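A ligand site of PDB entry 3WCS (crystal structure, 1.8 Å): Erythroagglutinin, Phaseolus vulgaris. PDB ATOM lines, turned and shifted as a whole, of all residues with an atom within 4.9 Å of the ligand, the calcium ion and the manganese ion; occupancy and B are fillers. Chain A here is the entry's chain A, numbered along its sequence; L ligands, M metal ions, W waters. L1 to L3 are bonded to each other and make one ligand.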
ATOM      1  N   ASP A  86       6.651  19.694   8.874  1.00  0.00           N
ATOM      2  CA  ASP A  86       7.110  18.923  10.062  1.00  0.00           C
ATOM      3  C   ASP A  86       7.374  19.834  11.247  1.00  0.00           C
ATOM      4  O   ASP A  86       7.454  19.375  12.408  1.00  0.00           O
ATOM      5  CB  ASP A  86       8.417  18.202   9.721  1.00  0.00           C
ATOM      6  CG  ASP A  86       8.191  16.813   9.221  1.00  0.00           C
ATOM      7  OD1 ASP A  86       7.917  15.922  10.073  1.00  0.00           O
ATOM      8  OD2 ASP A  86       8.333  16.581   7.994  1.00  0.00           O
ATOM      9  N   LYS A 102      16.162  16.156   6.003  1.00  0.00           N
ATOM     10  CA  LYS A 102      14.882  16.862   5.958  1.00  0.00           C
ATOM     11  C   LYS A 102      13.770  16.175   6.763  1.00  0.00           C
ATOM     12  O   LYS A 102      14.030  15.321   7.634  1.00  0.00           O
ATOM     13  CB  LYS A 102      14.463  17.060   4.495  1.00  0.00           C
ATOM     14  CG  LYS A 102      14.177  15.754   3.746  1.00  0.00           C
ATOM     15  CD  LYS A 102      13.656  16.011   2.330  1.00  0.00           C
ATOM     16  CE  LYS A 102      14.796  16.149   1.332  1.00  0.00           C
ATOM     17  NZ  LYS A 102      14.288  16.583  -0.003  1.00  0.00           N
ATOM     18  N   GLY A 103      12.527  16.568   6.502  1.00  0.00           N
ATOM     19  CA  GLY A 103      11.384  15.965   7.210  1.00  0.00           C
ATOM     20  C   GLY A 103      11.451  16.118   8.731  1.00  0.00           C
ATOM     21  O   GLY A 103      11.735  17.186   9.257  1.00  0.00           O
ATOM     22  N   GLY A 104      11.216  15.004   9.443  1.00  0.00           N
ATOM     23  CA  GLY A 104      11.155  15.060  10.896  1.00  0.00           C
ATOM     24  C   GLY A 104      12.484  15.392  11.585  1.00  0.00           C
ATOM     25  O   GLY A 104      12.520  15.664  12.761  1.00  0.00           O
ATOM     26  N   LEU A 105      13.573  15.342  10.848  1.00  0.00           N
ATOM     27  CA  LEU A 105      14.864  15.690  11.425  1.00  0.00           C
ATOM     28  C   LEU A 105      15.160  17.202  11.319  1.00  0.00           C
ATOM     29  O   LEU A 105      16.192  17.682  11.817  1.00  0.00           O
ATOM     30  CB  LEU A 105      15.959  14.844  10.772  1.00  0.00           C
ATOM     31  CG  LEU A 105      15.788  13.328  11.035  1.00  0.00           C
ATOM     32  CD1 LEU A 105      16.769  12.495  10.213  1.00  0.00           C
ATOM     33  CD2 LEU A 105      15.863  13.001  12.521  1.00  0.00           C
ATOM     34  N   TYR A 112      18.119   9.842  14.426  1.00  0.00           N
ATOM     35  CA  TYR A 112      17.519  10.235  15.701  1.00  0.00           C
ATOM     36  C   TYR A 112      18.306   9.820  16.952  1.00  0.00           C
ATOM     37  O   TYR A 112      17.757   9.789  18.049  1.00  0.00           O
ATOM     38  CB  TYR A 112      16.045   9.817  15.789  1.00  0.00           C
ATOM     39  CG  TYR A 112      15.718   8.355  15.514  1.00  0.00           C
ATOM     40  CD1 TYR A 112      15.626   7.423  16.554  1.00  0.00           C
ATOM     41  CD2 TYR A 112      15.439   7.920  14.217  1.00  0.00           C
ATOM     42  CE1 TYR A 112      15.297   6.087  16.303  1.00  0.00           C
ATOM     43  CE2 TYR A 112      15.096   6.595  13.951  1.00  0.00           C
ATOM     44  CZ  TYR A 112      15.036   5.688  14.994  1.00  0.00           C
ATOM     45  OH  TYR A 112      14.688   4.388  14.696  1.00  0.00           O
ATOM     46  N   GLU A 124      12.324  23.700  19.271  1.00  0.00           N
ATOM     47  CA  GLU A 124      11.498  23.214  18.170  1.00  0.00           C
ATOM     48  C   GLU A 124      10.011  23.382  18.409  1.00  0.00           C
ATOM     49  O   GLU A 124       9.541  23.334  19.551  1.00  0.00           O
ATOM     50  CB  GLU A 124      11.792  21.746  17.844  1.00  0.00           C
ATOM     51  CG  GLU A 124      11.459  20.758  18.989  1.00  0.00           C
ATOM     52  CD  GLU A 124      11.414  19.295  18.524  1.00  0.00           C
ATOM     53  OE1 GLU A 124      12.437  18.868  17.920  1.00  0.00           O
ATOM     54  OE2 GLU A 124      10.394  18.556  18.728  1.00  0.00           O
ATOM     55  N   ASP A 126       7.090  21.553  16.897  1.00  0.00           N
ATOM     56  CA  ASP A 126       7.018  20.261  16.148  1.00  0.00           C
ATOM     57  C   ASP A 126       5.540  19.916  15.922  1.00  0.00           C
ATOM     58  O   ASP A 126       4.779  19.743  16.877  1.00  0.00           O
ATOM     59  CB  ASP A 126       7.749  19.168  16.986  1.00  0.00           C
ATOM     60  CG  ASP A 126       7.946  17.823  16.246  1.00  0.00           C
ATOM     61  OD1 ASP A 126       7.281  17.640  15.209  1.00  0.00           O
ATOM     62  OD2 ASP A 126       8.788  16.948  16.707  1.00  0.00           O
ATOM     63  N   LEU A 128       4.398  17.364  13.821  1.00  0.00           N
ATOM     64  CA  LEU A 128       4.211  15.999  13.303  1.00  0.00           C
ATOM     65  C   LEU A 128       4.829  14.977  14.254  1.00  0.00           C
ATOM     66  O   LEU A 128       6.020  15.000  14.539  1.00  0.00           O
ATOM     67  CB  LEU A 128       4.818  15.851  11.902  1.00  0.00           C
ATOM     68  CG  LEU A 128       4.364  14.446  11.421  1.00  0.00           C
ATOM     69  CD1 LEU A 128       3.422  14.403  10.222  1.00  0.00           C
ATOM     70  CD2 LEU A 128       5.490  13.405  11.441  1.00  0.00           C
ATOM     71  N   TYR A 129       3.976  14.059  14.711  1.00  0.00           N
ATOM     72  CA  TYR A 129       4.426  12.965  15.607  1.00  0.00           C
ATOM     73  C   TYR A 129       5.288  11.941  14.875  1.00  0.00           C
ATOM     74  O   TYR A 129       4.803  11.242  13.967  1.00  0.00           O
ATOM     75  CB  TYR A 129       3.182  12.312  16.180  1.00  0.00           C
ATOM     76  CG  TYR A 129       3.388  10.934  16.807  1.00  0.00           C
ATOM     77  CD1 TYR A 129       4.264  10.761  17.850  1.00  0.00           C
ATOM     78  CD2 TYR A 129       2.724   9.829  16.301  1.00  0.00           C
ATOM     79  CE1 TYR A 129       4.429   9.487  18.425  1.00  0.00           C
ATOM     80  CE2 TYR A 129       2.879   8.560  16.854  1.00  0.00           C
ATOM     81  CZ  TYR A 129       3.735   8.401  17.904  1.00  0.00           C
ATOM     82  OH  TYR A 129       3.886   7.123  18.447  1.00  0.00           O
ATOM     83  N   ASN A 130       6.560  11.843  15.272  1.00  0.00           N
ATOM     84  CA  ASN A 130       7.484  10.906  14.655  1.00  0.00           C
ATOM     85  C   ASN A 130       7.607   9.765  15.651  1.00  0.00           C
ATOM     86  O   ASN A 130       8.140   9.934  16.737  1.00  0.00           O
ATOM     87  CB  ASN A 130       8.843  11.565  14.385  1.00  0.00           C
ATOM     88  CG  ASN A 130       8.799  12.519  13.197  1.00  0.00           C
ATOM     89  OD1 ASN A 130       8.774  13.756  13.365  1.00  0.00           O
ATOM     90  ND2 ASN A 130       8.805  11.941  11.989  1.00  0.00           N
ATOM     91  N   VAL A 131       7.061   8.615  15.272  1.00  0.00           N
ATOM     92  CA  VAL A 131       6.883   7.485  16.201  1.00  0.00           C
ATOM     93  C   VAL A 131       8.120   7.047  16.978  1.00  0.00           C
ATOM     94  O   VAL A 131       8.018   6.586  18.125  1.00  0.00           O
ATOM     95  CB  VAL A 131       6.243   6.284  15.439  1.00  0.00           C
ATOM     96  CG1 VAL A 131       7.162   5.773  14.336  1.00  0.00           C
ATOM     97  CG2 VAL A 131       5.864   5.168  16.398  1.00  0.00           C
ATOM     98  N   HIS A 132       9.291   7.191  16.380  1.00  0.00           N
ATOM     99  CA  HIS A 132      10.519   6.668  17.007  1.00  0.00           C
ATOM    100  C   HIS A 132      11.124   7.546  18.071  1.00  0.00           C
ATOM    101  O   HIS A 132      12.037   7.128  18.801  1.00  0.00           O
ATOM    102  CB  HIS A 132      11.559   6.300  15.951  1.00  0.00           C
ATOM    103  CG  HIS A 132      11.097   5.238  14.983  1.00  0.00           C
ATOM    104  ND1 HIS A 132      10.680   4.009  15.381  1.00  0.00           N
ATOM    105  CD2 HIS A 132      11.058   5.234  13.583  1.00  0.00           C
ATOM    106  CE1 HIS A 132      10.341   3.272  14.307  1.00  0.00           C
ATOM    107  NE2 HIS A 132      10.575   4.015  13.193  1.00  0.00           N
ATOM    108  N   TRP A 133      10.640   8.791  18.199  1.00  0.00           N
ATOM    109  CA  TRP A 133      11.190   9.711  19.204  1.00  0.00           C
ATOM    110  C   TRP A 133      10.292  10.741  19.844  1.00  0.00           C
ATOM    111  O   TRP A 133      10.594  11.222  20.913  1.00  0.00           O
ATOM    112  CB  TRP A 133      12.458  10.389  18.669  1.00  0.00           C
ATOM    113  CG  TRP A 133      12.171  11.356  17.540  1.00  0.00           C
ATOM    114  CD1 TRP A 133      11.727  12.666  17.650  1.00  0.00           C
ATOM    115  CD2 TRP A 133      12.363  11.125  16.116  1.00  0.00           C
ATOM    116  NE1 TRP A 133      11.588  13.241  16.393  1.00  0.00           N
ATOM    117  CE2 TRP A 133      11.972  12.375  15.435  1.00  0.00           C
ATOM    118  CE3 TRP A 133      12.779  10.044  15.339  1.00  0.00           C
ATOM    119  CZ2 TRP A 133      12.018  12.503  14.068  1.00  0.00           C
ATOM    120  CZ3 TRP A 133      12.819  10.188  13.959  1.00  0.00           C
ATOM    121  CH2 TRP A 133      12.436  11.394  13.337  1.00  0.00           C
ATOM    122  N   ASP A 134       9.201  11.133  19.183  1.00  0.00           N
ATOM    123  CA  ASP A 134       8.344  12.219  19.681  1.00  0.00           C
ATOM    124  C   ASP A 134       7.256  11.769  20.669  1.00  0.00           C
ATOM    125  O   ASP A 134       6.750  10.663  20.538  1.00  0.00           O
ATOM    126  CB  ASP A 134       7.605  12.881  18.501  1.00  0.00           C
ATOM    127  CG  ASP A 134       8.450  13.947  17.772  1.00  0.00           C
ATOM    128  OD1 ASP A 134       9.273  14.695  18.399  1.00  0.00           O
ATOM    129  OD2 ASP A 134       8.199  14.066  16.539  1.00  0.00           O
ATOM    130  N   PRO A 135       6.838  12.669  21.599  1.00  0.00           N
ATOM    131  CA  PRO A 135       5.555  12.519  22.281  1.00  0.00           C
ATOM    132  C   PRO A 135       4.449  12.669  21.233  1.00  0.00           C
ATOM    133  O   PRO A 135       4.652  13.335  20.216  1.00  0.00           O
ATOM    134  CB  PRO A 135       5.528  13.678  23.280  1.00  0.00           C
ATOM    135  CG  PRO A 135       6.465  14.703  22.725  1.00  0.00           C
ATOM    136  CD  PRO A 135       7.483  13.981  21.895  1.00  0.00           C
ATOM    137  N   HIS A 139       4.064  19.721  20.057  1.00  0.00           N
ATOM    138  CA  HIS A 139       4.859  20.102  21.220  1.00  0.00           C
ATOM    139  C   HIS A 139       5.889  21.159  20.912  1.00  0.00           C
ATOM    140  O   HIS A 139       6.326  21.320  19.758  1.00  0.00           O
ATOM    141  CB  HIS A 139       5.554  18.844  21.822  1.00  0.00           C
ATOM    142  CG  HIS A 139       6.369  18.034  20.833  1.00  0.00           C
ATOM    143  ND1 HIS A 139       5.813  17.124  20.004  1.00  0.00           N
ATOM    144  CD2 HIS A 139       7.739  18.077  20.523  1.00  0.00           C
ATOM    145  CE1 HIS A 139       6.783  16.571  19.236  1.00  0.00           C
ATOM    146  NE2 HIS A 139       7.980  17.167  19.534  1.00  0.00           N
ATOM    147  N   ILE A 147      17.450  15.079  17.972  1.00  0.00           N
ATOM    148  CA  ILE A 147      16.035  15.342  17.651  1.00  0.00           C
ATOM    149  C   ILE A 147      15.118  14.850  18.781  1.00  0.00           C
ATOM    150  O   ILE A 147      13.955  15.248  18.868  1.00  0.00           O
ATOM    151  CB  ILE A 147      15.623  14.760  16.275  1.00  0.00           C
ATOM    152  CG1 ILE A 147      14.343  15.423  15.740  1.00  0.00           C
ATOM    153  CG2 ILE A 147      15.373  13.250  16.381  1.00  0.00           C
ATOM    154  CD1 ILE A 147      14.505  16.892  15.342  1.00  0.00           C
ATOM    155  N   SER A 149      13.979  15.442  22.075  1.00  0.00           N
ATOM    156  CA  SER A 149      14.079  16.647  22.936  1.00  0.00           C
ATOM    157  C   SER A 149      14.409  16.266  24.356  1.00  0.00           C
ATOM    158  O   SER A 149      13.879  15.273  24.842  1.00  0.00           O
ATOM    159  CB  SER A 149      12.765  17.419  22.935  1.00  0.00           C
ATOM    160  OG  SER A 149      12.425  17.775  21.603  1.00  0.00           O
ATOM    161  N   GLY A 214       6.543  18.057   5.272  1.00  0.00           N
ATOM    162  CA  GLY A 214       6.419  16.605   5.271  1.00  0.00           C
ATOM    163  C   GLY A 214       6.895  15.999   3.963  1.00  0.00           C
ATOM    164  O   GLY A 214       6.839  16.647   2.909  1.00  0.00           O
ATOM    165  N   ILE A 215       7.369  14.769   4.019  1.00  0.00           N
ATOM    166  CA  ILE A 215       7.819  14.106   2.798  1.00  0.00           C
ATOM    167  C   ILE A 215       6.701  13.305   2.122  1.00  0.00           C
ATOM    168  O   ILE A 215       6.831  12.904   0.968  1.00  0.00           O
ATOM    169  CB  ILE A 215       9.087  13.253   3.009  1.00  0.00           C
ATOM    170  CG1 ILE A 215       8.823  12.056   3.955  1.00  0.00           C
ATOM    171  CG2 ILE A 215      10.225  14.106   3.546  1.00  0.00           C
ATOM    172  CD1 ILE A 215       9.924  11.007   3.912  1.00  0.00           C
ATOM    173  N   THR A 216       5.603  13.090   2.848  1.00  0.00           N
ATOM    174  CA  THR A 216       4.487  12.266   2.387  1.00  0.00           C
ATOM    175  C   THR A 216       3.261  13.132   2.126  1.00  0.00           C
ATOM    176  O   THR A 216       2.874  13.943   2.986  1.00  0.00           O
ATOM    177  CB  THR A 216       4.119  11.210   3.447  1.00  0.00           C
ATOM    178  OG1 THR A 216       5.270  10.400   3.706  1.00  0.00           O
ATOM    179  CG2 THR A 216       2.982  10.326   2.970  1.00  0.00           C
ATOM    180  N   ASN A 219       0.817  15.813   4.444  1.00  0.00           N
ATOM    181  CA  ASN A 219       1.548  16.336   5.610  1.00  0.00           C
ATOM    182  C   ASN A 219       2.452  17.471   5.137  1.00  0.00           C
ATOM    183  O   ASN A 219       3.542  17.241   4.635  1.00  0.00           O
ATOM    184  CB  ASN A 219       2.418  15.238   6.242  1.00  0.00           C
ATOM    185  CG  ASN A 219       1.606  14.003   6.607  1.00  0.00           C
ATOM    186  OD1 ASN A 219       1.018  13.945   7.685  1.00  0.00           O
ATOM    187  ND2 ASN A 219       1.551  13.040   5.700  1.00  0.00           N
HETATM  188  C1  LIG L   1      10.412   9.040   7.587  1.00  0.00           C
HETATM  189  C2  LIG L   1       9.763  10.417   7.679  1.00  0.00           C
HETATM  190  C3  LIG L   1      10.849  11.472   7.963  1.00  0.00           C
HETATM  191  C4  LIG L   1      11.573  11.130   9.262  1.00  0.00           C
HETATM  192  C5  LIG L   1      12.188   9.741   9.104  1.00  0.00           C
HETATM  193  C6  LIG L   1      12.939   9.266  10.345  1.00  0.00           C
HETATM  194  O1  LIG L   1      11.248   8.966   6.448  1.00  0.00           O
HETATM  195  O2  LIG L   1       8.870  10.447   8.770  1.00  0.00           O
HETATM  196  O3  LIG L   1      10.218  12.734   8.086  1.00  0.00           O
HETATM  197  O4  LIG L   1      12.563  12.101   9.595  1.00  0.00           O
HETATM  198  O5  LIG L   1      11.154   8.799   8.792  1.00  0.00           O
HETATM  199  O6  LIG L   1      13.671   8.092  10.015  1.00  0.00           O
HETATM  200  C1  LG2 L   2       7.516  10.150   8.376  1.00  0.00           C
HETATM  201  C2  LG2 L   2       6.836   9.482   9.574  1.00  0.00           C
HETATM  202  C3  LG2 L   2       5.377   9.201   9.239  1.00  0.00           C
HETATM  203  C4  LG2 L   2       4.652  10.447   8.732  1.00  0.00           C
HETATM  204  C5  LG2 L   2       5.454  11.096   7.593  1.00  0.00           C
HETATM  205  C6  LG2 L   2       4.877  12.440   7.164  1.00  0.00           C
HETATM  206  C7  LG2 L   2       8.324   8.072  10.919  1.00  0.00           C
HETATM  207  C8  LG2 L   2       8.963   6.714  11.048  1.00  0.00           C
HETATM  208  N1  LG2 L   2       7.536   8.237   9.866  1.00  0.00           N
HETATM  209  O1  LG2 L   2       4.721   8.675  10.374  1.00  0.00           O
HETATM  210  O2  LG2 L   2       3.392   9.992   8.255  1.00  0.00           O
HETATM  211  O3  LG2 L   2       6.797  11.320   8.000  1.00  0.00           O
HETATM  212  O4  LG2 L   2       5.664  12.934   6.087  1.00  0.00           O
HETATM  213  O5  LG2 L   2       8.555   8.954  11.758  1.00  0.00           O
HETATM  214  C1  LG3 L   3       2.303  10.721   8.813  1.00  0.00           C
HETATM  215  C2  LG3 L   3       1.022  10.145   8.215  1.00  0.00           C
HETATM  216  C3  LG3 L   3      -0.183  10.797   8.885  1.00  0.00           C
HETATM  217  C4  LG3 L   3      -0.083  10.692  10.404  1.00  0.00           C
HETATM  218  C5  LG3 L   3       1.250  11.259  10.907  1.00  0.00           C
HETATM  219  C6  LG3 L   3       1.491  11.031  12.402  1.00  0.00           C
HETATM  220  O1  LG3 L   3       1.021  10.317   6.805  1.00  0.00           O
HETATM  221  O2  LG3 L   3      -1.374  10.173   8.437  1.00  0.00           O
HETATM  222  O3  LG3 L   3      -0.136   9.320  10.765  1.00  0.00           O
HETATM  223  O4  LG3 L   3       2.290  10.597  10.224  1.00  0.00           O
HETATM  224  O5  LG3 L   3       0.573  11.705  13.217  1.00  0.00           O
HETATM  225 CA    CA M   1       8.293  15.567  14.780  1.00  0.00          CA
HETATM  226 MN    MN M   2       9.669  16.668  18.525  1.00  0.00          MN
HETATM  227  O   HOH W   1      14.222  12.586   7.507  1.00  0.00           O
HETATM  228  O   HOH W   2       7.062   6.053   8.104  1.00  0.00           O
HETATM  229  O   HOH W   3       8.263  16.786  12.822  1.00  0.00           O
HETATM  230  O   HOH W   4      12.630   5.563  10.546  1.00  0.00           O
HETATM  231  O   HOH W   5       8.112  14.114   6.682  1.00  0.00           O
HETATM  232  O   HOH W   6       5.126   8.677  13.042  1.00  0.00           O
HETATM  233  O   HOH W   7       1.120  14.254  14.049  1.00  0.00           O
HETATM  234  O   HOH W   8      10.149   8.349  13.863  1.00  0.00           O
HETATM  235  O   HOH W   9      11.395  16.448  17.613  1.00  0.00           O
HETATM  236  O   HOH W  10      10.538  16.038  20.213  1.00  0.00           O
HETATM  237  O   HOH W  11       8.202  13.340   9.773  1.00  0.00           O
HETATM  238  O   HOH W  12       2.058   7.588  10.720  1.00  0.00           O
HETATM  239  O   HOH W  13      16.315   8.504  10.881  1.00  0.00           O
HETATM  240  O   HOH W  14      10.602  15.831  15.011  1.00  0.00           O
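Within 4 Å of the calcium ion: Asp 126, Leu 128, Asn 130 and Asp 134.
The calcium ion is bound by water W3 (2.3 Å), the side-chain carboxylate (OD2) of Asp 134 (2.3 Å), water W14 (2.3 Å), the side-chain carboxylate (OD1) of Asp 126 (2.3 Å), the side-chain amide oxygen (OD1) of Asn 130 (2.3 Å), the backbone carbonyl oxygen (O) of Leu 128 (2.4 Å) and the side-chain carboxylate (OD2) of Asp 126 (2.4 Å).
NE1 of Trp 133 sits close to OD1 of Asp 134, 3.4 Å away.
N of Gly 104 sits close to OD1 of Asp 86 (3.5 Å).
The backbone carbonyl oxygen (O) of Thr 216 lies within hydrogen-bond range of the side-chain amide nitrogen (ND2) of Asn 219 (3.2 Å).
The backbone NH (N) of Gly 214 sits close to the backbone carbonyl oxygen (O) of Asn 219.
O5 of LG2 L2 sits at hydrogen-bond distance from ND2 of Asn 130 (3.0 Å).
N of Gly 104 is in hydrogen-bond range of O3 of LIG L1, 2.8 Å away.
The side-chain amide nitrogen of Asn 219 sits at hydrogen-bond distance from an oxygen (O1) of LG3 L3 (3.0 Å).
The backbone NH (N) of Thr 216 lies within hydrogen-bond range of an oxygen (O4) of LG2 L2.
The side-chain hydroxyl (OG1) of Thr 216 is in hydrogen-bond range of an oxygen (O4) of LG2 L2 (3.5 Å).
N of Ile 215 lies within hydrogen-bond range of O4 of LG2 L2 (3.2 Å).
Residues that only touch the ligand: Gly 103 (3.5 Å), Leu 105 (3.6 Å), Tyr 129 (3.7 Å), Val 131 (3.8 Å), His 132 (3.6 Å), Trp 133 (3.7 Å) and Gly 214 (3.8 Å).
Hydrophobic or aromatic side chains that line the ligand: Leu 105, Leu 128, Tyr 129, Val 131, His 132, Trp 133 and Ile 215.
Of the 23 residues printed, 13 come within 4 Å of the ligand.
The nearest printed residue that does not touch the ligand is Lys 102 (4.05 Å).
The manganese ion is bound by water W9, water W10, the side-chain carboxylate of Asp 134, a ring nitrogen (NE2) of His 139, the side-chain carboxylate of Glu 124 and the side-chain carboxylate of Asp 126.
Of the 23 residues printed, 4 come within 4 Å of the manganese ion.
The nearest printed residue that does not touch the manganese ion is Ser 149 (4.3 Å).
Water W14 bridges the backbone carbonyl oxygen (O) of Gly 104 (3.0 Å) and the indole nitrogen (NE1) of Trp 133 (3.1 Å).
Water W9 lies within hydrogen-bond range of the side-chain carboxylate of Glu 124 (2.7 Å), the backbone carbonyl oxygen of Ile 147 (3.1 Å) and the indole nitrogen of Trp 133 (3.4 Å).
Water W6 lies within hydrogen-bond range of an oxygen (O1) of LG2 L2, the backbone carbonyl oxygen of Tyr 129 and the backbone NH of Val 131.
Water W11 lies within hydrogen-bond range of OD1 of Asp 86 (2.6 Å), ND2 of Asn 130 (2.7 Å), O3 of LIG L1 (2.7 Å) and N of Gly 104 (3.5 Å).
Water W8 lies within hydrogen-bond range of O5 of LG2 L2, N of His 132 and N of Val 131.
Water W1 bridges O4 of LIG L1 (2.7 Å) and O of Lys 102 (2.7 Å).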
